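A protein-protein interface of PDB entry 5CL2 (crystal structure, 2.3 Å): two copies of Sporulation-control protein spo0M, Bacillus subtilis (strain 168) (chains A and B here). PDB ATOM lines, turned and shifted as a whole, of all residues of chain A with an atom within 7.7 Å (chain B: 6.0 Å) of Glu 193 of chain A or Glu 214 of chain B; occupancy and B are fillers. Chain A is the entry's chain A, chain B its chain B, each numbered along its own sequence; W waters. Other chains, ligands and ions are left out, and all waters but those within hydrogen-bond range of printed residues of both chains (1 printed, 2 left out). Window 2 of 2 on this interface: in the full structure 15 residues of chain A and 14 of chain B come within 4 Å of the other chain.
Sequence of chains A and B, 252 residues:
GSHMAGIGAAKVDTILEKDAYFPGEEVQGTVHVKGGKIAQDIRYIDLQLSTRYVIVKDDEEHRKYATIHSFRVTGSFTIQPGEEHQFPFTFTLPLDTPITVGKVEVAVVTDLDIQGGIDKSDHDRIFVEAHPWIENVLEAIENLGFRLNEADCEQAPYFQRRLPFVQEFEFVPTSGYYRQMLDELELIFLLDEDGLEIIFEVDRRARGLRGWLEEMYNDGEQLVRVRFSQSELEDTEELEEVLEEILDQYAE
The backbone NH of Leu 95 of chain A lies within hydrogen-bond range of the side-chain amide oxygen of Gln 160 of chain B, 3.2 Å away. OD1 of Asp 192 of chain A is in salt-bridge range of NH1 of Arg 225 of chain B (3.5 Å). The side-chain hydroxyl of Tyr 158 of chain B lies within hydrogen-bond range of the side-chain carboxylate of Asp 194 of chain A (2.9 Å). NE2 of Gln 222 of chain B is in hydrogen-bond range of OE1 of Gln 230 of chain A, at 3.1 Å.
N of Asp 194 of chain A lies within hydrogen-bond range of OD1 of Asp 192 of chain A, 3.2 Å away. The side-chain carboxylate (OD1) of Asp 192 of chain A sits at hydrogen-bond distance from the backbone NH (N) of Gly 195 of chain A, 3.3 Å away. The side-chain carboxylate (OD1) of Asp 192 of chain A is in salt-bridge range of the guanidinium group (NH2) of Arg 227 of chain A, 2.6 Å away. The backbone NH (N) of Gln 230 of chain A sits at hydrogen-bond distance from the backbone carbonyl oxygen (O) of Asp 194 of chain A (3.4 Å). N of Tyr 158 of chain B sits at hydrogen-bond distance from O of Trp 212 of chain B, 3.2 Å away.
Among the printed residues, merely in contact across the chains: Glu 193 of chain A with Tyr 158 of chain B, Arg 227 of chain A with Arg 225 of chain B, Glu 193 of chain A with Gln 160 of chain B and Glu 193 of chain A with Glu 214 of chain B.
Printed residues of chain B within 4 Å of Asp 192 of chain A: Arg 225 (3.5 Å). Glu 193 of chain A touches just these residues of chain B: Tyr 158 (3.5 Å), Gln 160 (3.8 Å) and Glu 214 (3.9 Å). Of the printed residues of chain B, Arg 227 of chain A touches Arg 225. Of the printed residues of chain A, Tyr 158 of chain B touches Glu 193 and Asp 194. Printed residues of chain A within 4 Å of Gln 160 of chain B: Leu 95 and Glu 193. Of chain A, only Glu 193 (3.9 Å) comes within 4 Å of Glu 214 of chain B. Of the printed residues of chain A, Arg 225 of chain B touches Asp 192 and Arg 227. The nearest residue of chain B that does not touch Glu 193 of chain A is Gln 222 of chain B (5.3 Å). The nearest residue of chain A that does not touch Glu 214 of chain B is Thr 92 of chain A (5.8 Å). The nearest printed residue of chain A that does not touch Arg 225 of chain B is Asp 194 of chain A (4.9 Å).
Printed residues of chain A that touch a printed residue of chain B: Leu 95, Asp 192, Glu 193, Asp 194, Arg 227 and Gln 230. Along chain A the printed residues that touch a printed residue of chain B span positions 95 to 230. Of the 13 printed residues of chain B, 5 touch a printed residue of chain A. Printed residues of chain B that touch a printed residue of chain A: Tyr 158, Gln 160, Glu 214, Gln 222 and Arg 225. Hydrophobic or aromatic side chains of chain B that line the printed part of chain A: Tyr 158.
No position is printed for both chains.
Water W1 bridges NE2 of Gln 160 of chain B and O of Leu 93 of chain A.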
ATOM      1  N   PRO A  23       0.777  25.299 -19.850  1.00  0.00           N
ATOM      2  CA  PRO A  23       1.973  24.958 -19.068  1.00  0.00           C
ATOM      3  C   PRO A  23       2.703  26.162 -18.494  1.00  0.00           C
ATOM      4  O   PRO A  23       2.872  27.182 -19.173  1.00  0.00           O
ATOM      5  CB  PRO A  23       2.851  24.217 -20.084  1.00  0.00           C
ATOM      6  CG  PRO A  23       1.870  23.551 -20.966  1.00  0.00           C
ATOM      7  CD  PRO A  23       0.711  24.513 -21.095  1.00  0.00           C
ATOM      8  N   GLY A  24       3.121  26.036 -17.236  1.00  0.00           N
ATOM      9  CA  GLY A  24       3.848  27.099 -16.570  1.00  0.00           C
ATOM     10  C   GLY A  24       2.938  27.951 -15.707  1.00  0.00           C
ATOM     11  O   GLY A  24       3.391  28.625 -14.788  1.00  0.00           O
ATOM     12  N   THR A  92       2.365  24.572  -9.756  1.00  0.00           N
ATOM     13  CA  THR A  92       2.646  25.004 -11.099  1.00  0.00           C
ATOM     14  C   THR A  92       2.518  23.835 -12.050  1.00  0.00           C
ATOM     15  O   THR A  92       3.050  22.756 -11.789  1.00  0.00           O
ATOM     16  CB  THR A  92       4.038  25.613 -11.183  1.00  0.00           C
ATOM     17  OG1 THR A  92       4.151  26.621 -10.174  1.00  0.00           O
ATOM     18  CG2 THR A  92       4.277  26.228 -12.557  1.00  0.00           C
ATOM     19  N   LEU A  93       1.799  24.059 -13.143  1.00  0.00           N
ATOM     20  CA  LEU A  93       1.692  23.088 -14.226  1.00  0.00           C
ATOM     21  C   LEU A  93       3.063  22.924 -14.863  1.00  0.00           C
ATOM     22  O   LEU A  93       3.598  23.882 -15.431  1.00  0.00           O
ATOM     23  CB  LEU A  93       0.679  23.571 -15.255  1.00  0.00           C
ATOM     24  CG  LEU A  93      -0.295  22.596 -15.904  1.00  0.00           C
ATOM     25  CD1 LEU A  93      -1.272  22.092 -14.885  1.00  0.00           C
ATOM     26  CD2 LEU A  93      -1.026  23.262 -17.066  1.00  0.00           C
ATOM     27  N   LEU A  95       6.125  22.176 -17.404  1.00  0.00           N
ATOM     28  CA  LEU A  95       6.207  22.569 -18.814  1.00  0.00           C
ATOM     29  C   LEU A  95       6.039  21.407 -19.794  1.00  0.00           C
ATOM     30  O   LEU A  95       5.800  21.628 -20.991  1.00  0.00           O
ATOM     31  CB  LEU A  95       7.537  23.278 -19.083  1.00  0.00           C
ATOM     32  CG  LEU A  95       7.647  24.659 -18.432  1.00  0.00           C
ATOM     33  CD1 LEU A  95       8.973  25.359 -18.762  1.00  0.00           C
ATOM     34  CD2 LEU A  95       6.470  25.506 -18.876  1.00  0.00           C
ATOM     35  N   HIS A 131       0.684  26.453 -25.323  1.00  0.00           N
ATOM     36  CA  HIS A 131       1.467  27.612 -24.970  1.00  0.00           C
ATOM     37  C   HIS A 131       1.676  28.417 -26.253  1.00  0.00           C
ATOM     38  O   HIS A 131       1.843  27.838 -27.329  1.00  0.00           O
ATOM     39  CB  HIS A 131       2.783  27.143 -24.340  1.00  0.00           C
ATOM     40  CG  HIS A 131       3.730  28.235 -23.965  1.00  0.00           C
ATOM     41  ND1 HIS A 131       4.469  28.931 -24.901  1.00  0.00           N
ATOM     42  CD2 HIS A 131       4.123  28.703 -22.758  1.00  0.00           C
ATOM     43  CE1 HIS A 131       5.244  29.804 -24.287  1.00  0.00           C
ATOM     44  NE2 HIS A 131       5.053  29.686 -22.983  1.00  0.00           N
ATOM     45  N   TRP A 133       4.099  30.002 -27.836  1.00  0.00           N
ATOM     46  CA  TRP A 133       5.165  29.629 -28.777  1.00  0.00           C
ATOM     47  C   TRP A 133       4.763  28.418 -29.606  1.00  0.00           C
ATOM     48  O   TRP A 133       5.032  28.368 -30.813  1.00  0.00           O
ATOM     49  CB  TRP A 133       6.473  29.314 -28.060  1.00  0.00           C
ATOM     50  CG  TRP A 133       7.006  30.402 -27.171  1.00  0.00           C
ATOM     51  CD1 TRP A 133       6.666  31.724 -27.184  1.00  0.00           C
ATOM     52  CD2 TRP A 133       7.995  30.253 -26.150  1.00  0.00           C
ATOM     53  NE1 TRP A 133       7.377  32.404 -26.226  1.00  0.00           N
ATOM     54  CE2 TRP A 133       8.197  31.522 -25.573  1.00  0.00           C
ATOM     55  CE3 TRP A 133       8.714  29.164 -25.652  1.00  0.00           C
ATOM     56  CZ2 TRP A 133       9.092  31.732 -24.526  1.00  0.00           C
ATOM     57  CZ3 TRP A 133       9.599  29.372 -24.606  1.00  0.00           C
ATOM     58  CH2 TRP A 133       9.786  30.646 -24.058  1.00  0.00           C
ATOM     59  N   LEU A 190       9.288  20.075 -27.126  1.00  0.00           N
ATOM     60  CA  LEU A 190       9.841  20.013 -25.784  1.00  0.00           C
ATOM     61  C   LEU A 190      10.009  21.438 -25.276  1.00  0.00           C
ATOM     62  O   LEU A 190      10.934  22.155 -25.670  1.00  0.00           O
ATOM     63  CB  LEU A 190      11.177  19.273 -25.794  1.00  0.00           C
ATOM     64  CG  LEU A 190      11.162  17.948 -26.560  1.00  0.00           C
ATOM     65  CD1 LEU A 190      12.572  17.390 -26.716  1.00  0.00           C
ATOM     66  CD2 LEU A 190      10.276  16.960 -25.823  1.00  0.00           C
ATOM     67  N   LEU A 191       9.110  21.832 -24.386  1.00  0.00           N
ATOM     68  CA  LEU A 191       9.024  23.198 -23.929  1.00  0.00           C
ATOM     69  C   LEU A 191       9.834  23.373 -22.668  1.00  0.00           C
ATOM     70  O   LEU A 191       9.715  22.579 -21.738  1.00  0.00           O
ATOM     71  CB  LEU A 191       7.572  23.572 -23.684  1.00  0.00           C
ATOM     72  CG  LEU A 191       7.343  24.986 -23.181  1.00  0.00           C
ATOM     73  CD1 LEU A 191       7.732  25.955 -24.270  1.00  0.00           C
ATOM     74  CD2 LEU A 191       5.894  25.149 -22.803  1.00  0.00           C
ATOM     75  N   ASP A 192      10.672  24.400 -22.643  1.00  0.00           N
ATOM     76  CA  ASP A 192      11.373  24.790 -21.430  1.00  0.00           C
ATOM     77  C   ASP A 192      11.211  26.296 -21.240  1.00  0.00           C
ATOM     78  O   ASP A 192      10.459  26.946 -21.983  1.00  0.00           O
ATOM     79  CB  ASP A 192      12.844  24.348 -21.465  1.00  0.00           C
ATOM     80  CG  ASP A 192      13.607  24.885 -22.689  1.00  0.00           C
ATOM     81  OD1 ASP A 192      14.120  26.020 -22.624  1.00  0.00           O
ATOM     82  OD2 ASP A 192      13.687  24.160 -23.715  1.00  0.00           O
ATOM     83  N   GLU A 193      11.866  26.831 -20.212  1.00  0.00           N
ATOM     84  CA  GLU A 193      11.697  28.228 -19.807  1.00  0.00           C
ATOM     85  C   GLU A 193      12.284  29.242 -20.804  1.00  0.00           C
ATOM     86  O   GLU A 193      11.782  30.359 -20.944  1.00  0.00           O
ATOM     87  CB  GLU A 193      12.338  28.442 -18.426  1.00  0.00           C
ATOM     88  CG  GLU A 193      11.770  27.579 -17.281  1.00  0.00           C
ATOM     89  CD  GLU A 193      10.473  28.127 -16.701  1.00  0.00           C
ATOM     90  OE1 GLU A 193       9.951  29.122 -17.254  1.00  0.00           O
ATOM     91  OE2 GLU A 193       9.992  27.581 -15.674  1.00  0.00           O
ATOM     92  N   ASP A 194      13.377  28.873 -21.462  1.00  0.00           N
ATOM     93  CA  ASP A 194      14.076  29.821 -22.344  1.00  0.00           C
ATOM     94  C   ASP A 194      13.777  29.670 -23.821  1.00  0.00           C
ATOM     95  O   ASP A 194      14.258  30.446 -24.636  1.00  0.00           O
ATOM     96  CB  ASP A 194      15.580  29.718 -22.121  1.00  0.00           C
ATOM     97  CG  ASP A 194      15.940  29.931 -20.675  1.00  0.00           C
ATOM     98  OD1 ASP A 194      15.772  31.081 -20.206  1.00  0.00           O
ATOM     99  OD2 ASP A 194      16.376  28.954 -20.019  1.00  0.00           O
ATOM    100  N   GLY A 195      12.953  28.695 -24.159  1.00  0.00           N
ATOM    101  CA  GLY A 195      12.670  28.420 -25.544  1.00  0.00           C
ATOM    102  C   GLY A 195      12.018  27.073 -25.731  1.00  0.00           C
ATOM    103  O   GLY A 195      11.397  26.508 -24.816  1.00  0.00           O
ATOM    104  N   LEU A 196      12.158  26.553 -26.937  1.00  0.00           N
ATOM    105  CA  LEU A 196      11.408  25.380 -27.331  1.00  0.00           C
ATOM    106  C   LEU A 196      12.221  24.521 -28.296  1.00  0.00           C
ATOM    107  O   LEU A 196      12.857  25.043 -29.215  1.00  0.00           O
ATOM    108  CB  LEU A 196      10.100  25.842 -27.953  1.00  0.00           C
ATOM    109  CG  LEU A 196       9.050  24.849 -28.384  1.00  0.00           C
ATOM    110  CD1 LEU A 196       7.696  25.477 -28.218  1.00  0.00           C
ATOM    111  CD2 LEU A 196       9.311  24.540 -29.821  1.00  0.00           C
ATOM    112  N   ARG A 227      16.574  23.424 -31.883  1.00  0.00           N
ATOM    113  CA  ARG A 227      16.158  24.340 -30.821  1.00  0.00           C
ATOM    114  C   ARG A 227      15.888  25.755 -31.339  1.00  0.00           C
ATOM    115  O   ARG A 227      16.677  26.308 -32.101  1.00  0.00           O
ATOM    116  CB  ARG A 227      17.208  24.396 -29.713  1.00  0.00           C
ATOM    117  CG  ARG A 227      17.019  25.601 -28.814  1.00  0.00           C
ATOM    118  CD  ARG A 227      17.714  25.444 -27.483  1.00  0.00           C
ATOM    119  NE  ARG A 227      17.022  26.248 -26.486  1.00  0.00           N
ATOM    120  CZ  ARG A 227      16.107  25.757 -25.655  1.00  0.00           C
ATOM    121  NH1 ARG A 227      15.808  24.463 -25.686  1.00  0.00           N
ATOM    122  NH2 ARG A 227      15.504  26.556 -24.789  1.00  0.00           N
ATOM    123  N   GLN A 230      13.210  31.982 -27.478  1.00  0.00           N
ATOM    124  CA  GLN A 230      12.014  32.799 -27.304  1.00  0.00           C
ATOM    125  C   GLN A 230      11.841  33.853 -28.409  1.00  0.00           C
ATOM    126  O   GLN A 230      10.734  34.035 -28.931  1.00  0.00           O
ATOM    127  CB  GLN A 230      12.051  33.490 -25.944  1.00  0.00           C
ATOM    128  CG  GLN A 230      10.926  34.484 -25.716  1.00  0.00           C
ATOM    129  CD  GLN A 230      10.814  34.924 -24.256  1.00  0.00           C
ATOM    130  OE1 GLN A 230      11.750  34.752 -23.470  1.00  0.00           O
ATOM    131  NE2 GLN A 230       9.665  35.488 -23.893  1.00  0.00           N
ATOM    132  N   PRO B 157      16.296  22.532 -10.295  1.00  0.00           N
ATOM    133  CA  PRO B 157      14.845  22.468 -10.534  1.00  0.00           C
ATOM    134  C   PRO B 157      14.405  23.282 -11.744  1.00  0.00           C
ATOM    135  O   PRO B 157      13.420  22.924 -12.378  1.00  0.00           O
ATOM    136  CB  PRO B 157      14.238  23.042  -9.241  1.00  0.00           C
ATOM    137  CG  PRO B 157      15.327  23.865  -8.627  1.00  0.00           C
ATOM    138  CD  PRO B 157      16.607  23.144  -8.989  1.00  0.00           C
ATOM    139  N   TYR B 158      15.135  24.346 -12.060  1.00  0.00           N
ATOM    140  CA  TYR B 158      14.797  25.230 -13.178  1.00  0.00           C
ATOM    141  C   TYR B 158      14.658  24.500 -14.521  1.00  0.00           C
ATOM    142  O   TYR B 158      13.787  24.849 -15.328  1.00  0.00           O
ATOM    143  CB  TYR B 158      15.849  26.339 -13.298  1.00  0.00           C
ATOM    144  CG  TYR B 158      15.669  27.319 -14.451  1.00  0.00           C
ATOM    145  CD1 TYR B 158      14.680  28.299 -14.410  1.00  0.00           C
ATOM    146  CD2 TYR B 158      16.531  27.306 -15.549  1.00  0.00           C
ATOM    147  CE1 TYR B 158      14.530  29.214 -15.437  1.00  0.00           C
ATOM    148  CE2 TYR B 158      16.392  28.218 -16.586  1.00  0.00           C
ATOM    149  CZ  TYR B 158      15.392  29.169 -16.526  1.00  0.00           C
ATOM    150  OH  TYR B 158      15.251  30.077 -17.550  1.00  0.00           O
ATOM    151  N   GLN B 160      13.851  21.290 -15.017  1.00  0.00           N
ATOM    152  CA  GLN B 160      12.778  20.278 -14.999  1.00  0.00           C
ATOM    153  C   GLN B 160      13.165  19.019 -15.789  1.00  0.00           C
ATOM    154  O   GLN B 160      12.378  18.503 -16.588  1.00  0.00           O
ATOM    155  CB  GLN B 160      11.479  20.873 -15.553  1.00  0.00           C
ATOM    156  CG  GLN B 160      10.990  22.072 -14.749  1.00  0.00           C
ATOM    157  CD  GLN B 160       9.645  22.598 -15.207  1.00  0.00           C
ATOM    158  OE1 GLN B 160       8.812  21.861 -15.748  1.00  0.00           O
ATOM    159  NE2 GLN B 160       9.429  23.894 -14.999  1.00  0.00           N
ATOM    160  N   TRP B 212      20.659  25.629  -9.905  1.00  0.00           N
ATOM    161  CA  TRP B 212      19.985  26.254 -11.028  1.00  0.00           C
ATOM    162  C   TRP B 212      18.517  26.437 -10.704  1.00  0.00           C
ATOM    163  O   TRP B 212      17.741  25.481 -10.677  1.00  0.00           O
ATOM    164  CB  TRP B 212      20.193  25.431 -12.305  1.00  0.00           C
ATOM    165  CG  TRP B 212      21.637  25.307 -12.631  1.00  0.00           C
ATOM    166  CD1 TRP B 212      22.548  24.480 -12.036  1.00  0.00           C
ATOM    167  CD2 TRP B 212      22.360  26.074 -13.598  1.00  0.00           C
ATOM    168  NE1 TRP B 212      23.793  24.670 -12.594  1.00  0.00           N
ATOM    169  CE2 TRP B 212      23.703  25.643 -13.554  1.00  0.00           C
ATOM    170  CE3 TRP B 212      22.000  27.076 -14.507  1.00  0.00           C
ATOM    171  CZ2 TRP B 212      24.688  26.188 -14.378  1.00  0.00           C
ATOM    172  CZ3 TRP B 212      22.985  27.623 -15.320  1.00  0.00           C
ATOM    173  CH2 TRP B 212      24.310  27.165 -15.258  1.00  0.00           C
ATOM    174  N   LEU B 213      18.149  27.694 -10.485  1.00  0.00           N
ATOM    175  CA  LEU B 213      16.853  28.040  -9.925  1.00  0.00           C
ATOM    176  C   LEU B 213      16.196  29.175 -10.710  1.00  0.00           C
ATOM    177  O   LEU B 213      16.876  30.015 -11.301  1.00  0.00           O
ATOM    178  CB  LEU B 213      17.004  28.438  -8.446  1.00  0.00           C
ATOM    179  CG  LEU B 213      17.969  27.680  -7.523  1.00  0.00           C
ATOM    180  CD1 LEU B 213      18.180  28.421  -6.217  1.00  0.00           C
ATOM    181  CD2 LEU B 213      17.471  26.278  -7.237  1.00  0.00           C
ATOM    182  N   GLU B 214      14.868  29.195 -10.685  1.00  0.00           N
ATOM    183  CA  GLU B 214      14.044  30.213 -11.347  1.00  0.00           C
ATOM    184  C   GLU B 214      14.472  31.657 -11.079  1.00  0.00           C
ATOM    185  O   GLU B 214      14.467  32.509 -11.973  1.00  0.00           O
ATOM    186  CB  GLU B 214      12.606  30.062 -10.893  1.00  0.00           C
ATOM    187  CG  GLU B 214      11.649  29.631 -11.950  1.00  0.00           C
ATOM    188  CD  GLU B 214      10.313  29.369 -11.333  1.00  0.00           C
ATOM    189  OE1 GLU B 214      10.137  29.812 -10.173  1.00  0.00           O
ATOM    190  OE2 GLU B 214       9.456  28.733 -11.988  1.00  0.00           O
ATOM    191  N   GLU B 215      14.796  31.906  -9.816  1.00  0.00           N
ATOM    192  CA  GLU B 215      15.151  33.216  -9.283  1.00  0.00           C
ATOM    193  C   GLU B 215      16.367  33.843  -9.944  1.00  0.00           C
ATOM    194  O   GLU B 215      16.572  35.050  -9.863  1.00  0.00           O
ATOM    195  CB  GLU B 215      15.400  33.113  -7.758  1.00  0.00           C
ATOM    196  CG  GLU B 215      14.360  32.304  -6.913  1.00  0.00           C
ATOM    197  CD  GLU B 215      14.261  30.791  -7.232  1.00  0.00           C
ATOM    198  OE1 GLU B 215      14.779  30.344  -8.278  1.00  0.00           O
ATOM    199  OE2 GLU B 215      13.652  30.042  -6.435  1.00  0.00           O
ATOM    200  N   MET B 216      17.178  33.024 -10.593  1.00  0.00           N
ATOM    201  CA  MET B 216      18.330  33.524 -11.326  1.00  0.00           C
ATOM    202  C   MET B 216      17.962  34.092 -12.708  1.00  0.00           C
ATOM    203  O   MET B 216      18.703  34.905 -13.269  1.00  0.00           O
ATOM    204  CB  MET B 216      19.371  32.407 -11.445  1.00  0.00           C
ATOM    205  CG  MET B 216      19.676  31.767 -10.099  1.00  0.00           C
ATOM    206  SD  MET B 216      20.797  30.358 -10.065  1.00  0.00           S
ATOM    207  CE  MET B 216      20.969  30.126  -8.294  1.00  0.00           C
ATOM    208  N   TYR B 217      16.862  33.609 -13.282  1.00  0.00           N
ATOM    209  CA  TYR B 217      16.404  34.080 -14.592  1.00  0.00           C
ATOM    210  C   TYR B 217      15.122  34.956 -14.597  1.00  0.00           C
ATOM    211  O   TYR B 217      14.624  35.326 -15.666  1.00  0.00           O
ATOM    212  CB  TYR B 217      16.300  32.857 -15.502  1.00  0.00           C
ATOM    213  CG  TYR B 217      17.677  32.226 -15.565  1.00  0.00           C
ATOM    214  CD1 TYR B 217      18.643  32.720 -16.430  1.00  0.00           C
ATOM    215  CD2 TYR B 217      18.048  31.213 -14.680  1.00  0.00           C
ATOM    216  CE1 TYR B 217      19.917  32.188 -16.463  1.00  0.00           C
ATOM    217  CE2 TYR B 217      19.324  30.671 -14.699  1.00  0.00           C
ATOM    218  CZ  TYR B 217      20.259  31.165 -15.599  1.00  0.00           C
ATOM    219  OH  TYR B 217      21.542  30.649 -15.652  1.00  0.00           O
ATOM    220  N   ASN B 218      14.596  35.270 -13.409  1.00  0.00           N
ATOM    221  CA  ASN B 218      13.393  36.120 -13.252  1.00  0.00           C
ATOM    222  C   ASN B 218      13.584  37.630 -13.477  1.00  0.00           C
ATOM    223  O   ASN B 218      12.623  38.347 -13.767  1.00  0.00           O
ATOM    224  CB  ASN B 218      12.785  35.950 -11.847  1.00  0.00           C
ATOM    225  CG  ASN B 218      13.739  36.405 -10.726  1.00  0.00           C
ATOM    226  OD1 ASN B 218      14.670  37.192 -10.946  1.00  0.00           O
ATOM    227  ND2 ASN B 218      13.446  35.976  -9.502  1.00  0.00           N
ATOM    228  N   ASP B 219      14.819  38.101 -13.304  1.00  0.00           N
ATOM    229  CA  ASP B 219      15.146  39.527 -13.350  1.00  0.00           C
ATOM    230  C   ASP B 219      15.504  39.894 -14.794  1.00  0.00           C
ATOM    231  O   ASP B 219      15.989  40.991 -15.083  1.00  0.00           O
ATOM    232  CB  ASP B 219      16.291  39.841 -12.372  1.00  0.00           C
ATOM    233  CG  ASP B 219      16.747  41.295 -12.421  1.00  0.00           C
ATOM    234  OD1 ASP B 219      15.989  42.178 -11.964  1.00  0.00           O
ATOM    235  OD2 ASP B 219      17.868  41.555 -12.906  1.00  0.00           O
ATOM    236  N   GLN B 222      19.144  36.137 -19.072  1.00  0.00           N
ATOM    237  CA  GLN B 222      18.839  34.971 -19.889  1.00  0.00           C
ATOM    238  C   GLN B 222      20.074  34.152 -20.251  1.00  0.00           C
ATOM    239  O   GLN B 222      21.218  34.559 -20.035  1.00  0.00           O
ATOM    240  CB  GLN B 222      18.009  35.333 -21.130  1.00  0.00           C
ATOM    241  CG  GLN B 222      16.510  35.406 -20.775  1.00  0.00           C
ATOM    242  CD  GLN B 222      15.590  35.466 -21.974  1.00  0.00           C
ATOM    243  OE1 GLN B 222      15.974  35.943 -23.041  1.00  0.00           O
ATOM    244  NE2 GLN B 222      14.363  34.961 -21.809  1.00  0.00           N
ATOM    245  N   ARG B 225      21.687  28.608 -24.689  1.00  0.00           N
ATOM    246  CA  ARG B 225      21.395  27.187 -24.792  1.00  0.00           C
ATOM    247  C   ARG B 225      21.490  26.731 -26.231  1.00  0.00           C
ATOM    248  O   ARG B 225      20.731  27.185 -27.078  1.00  0.00           O
ATOM    249  CB  ARG B 225      20.012  26.898 -24.232  1.00  0.00           C
ATOM    250  CG  ARG B 225      19.822  25.465 -23.866  1.00  0.00           C
ATOM    251  CD  ARG B 225      18.656  25.298 -22.942  1.00  0.00           C
ATOM    252  NE  ARG B 225      18.181  23.924 -22.989  1.00  0.00           N
ATOM    253  CZ  ARG B 225      17.274  23.428 -22.155  1.00  0.00           C
ATOM    254  NH1 ARG B 225      16.761  24.199 -21.203  1.00  0.00           N
ATOM    255  NH2 ARG B 225      16.885  22.163 -22.270  1.00  0.00           N
HETATM  256  O   HOH W   1       6.921  24.657 -14.827  1.00  0.00           O
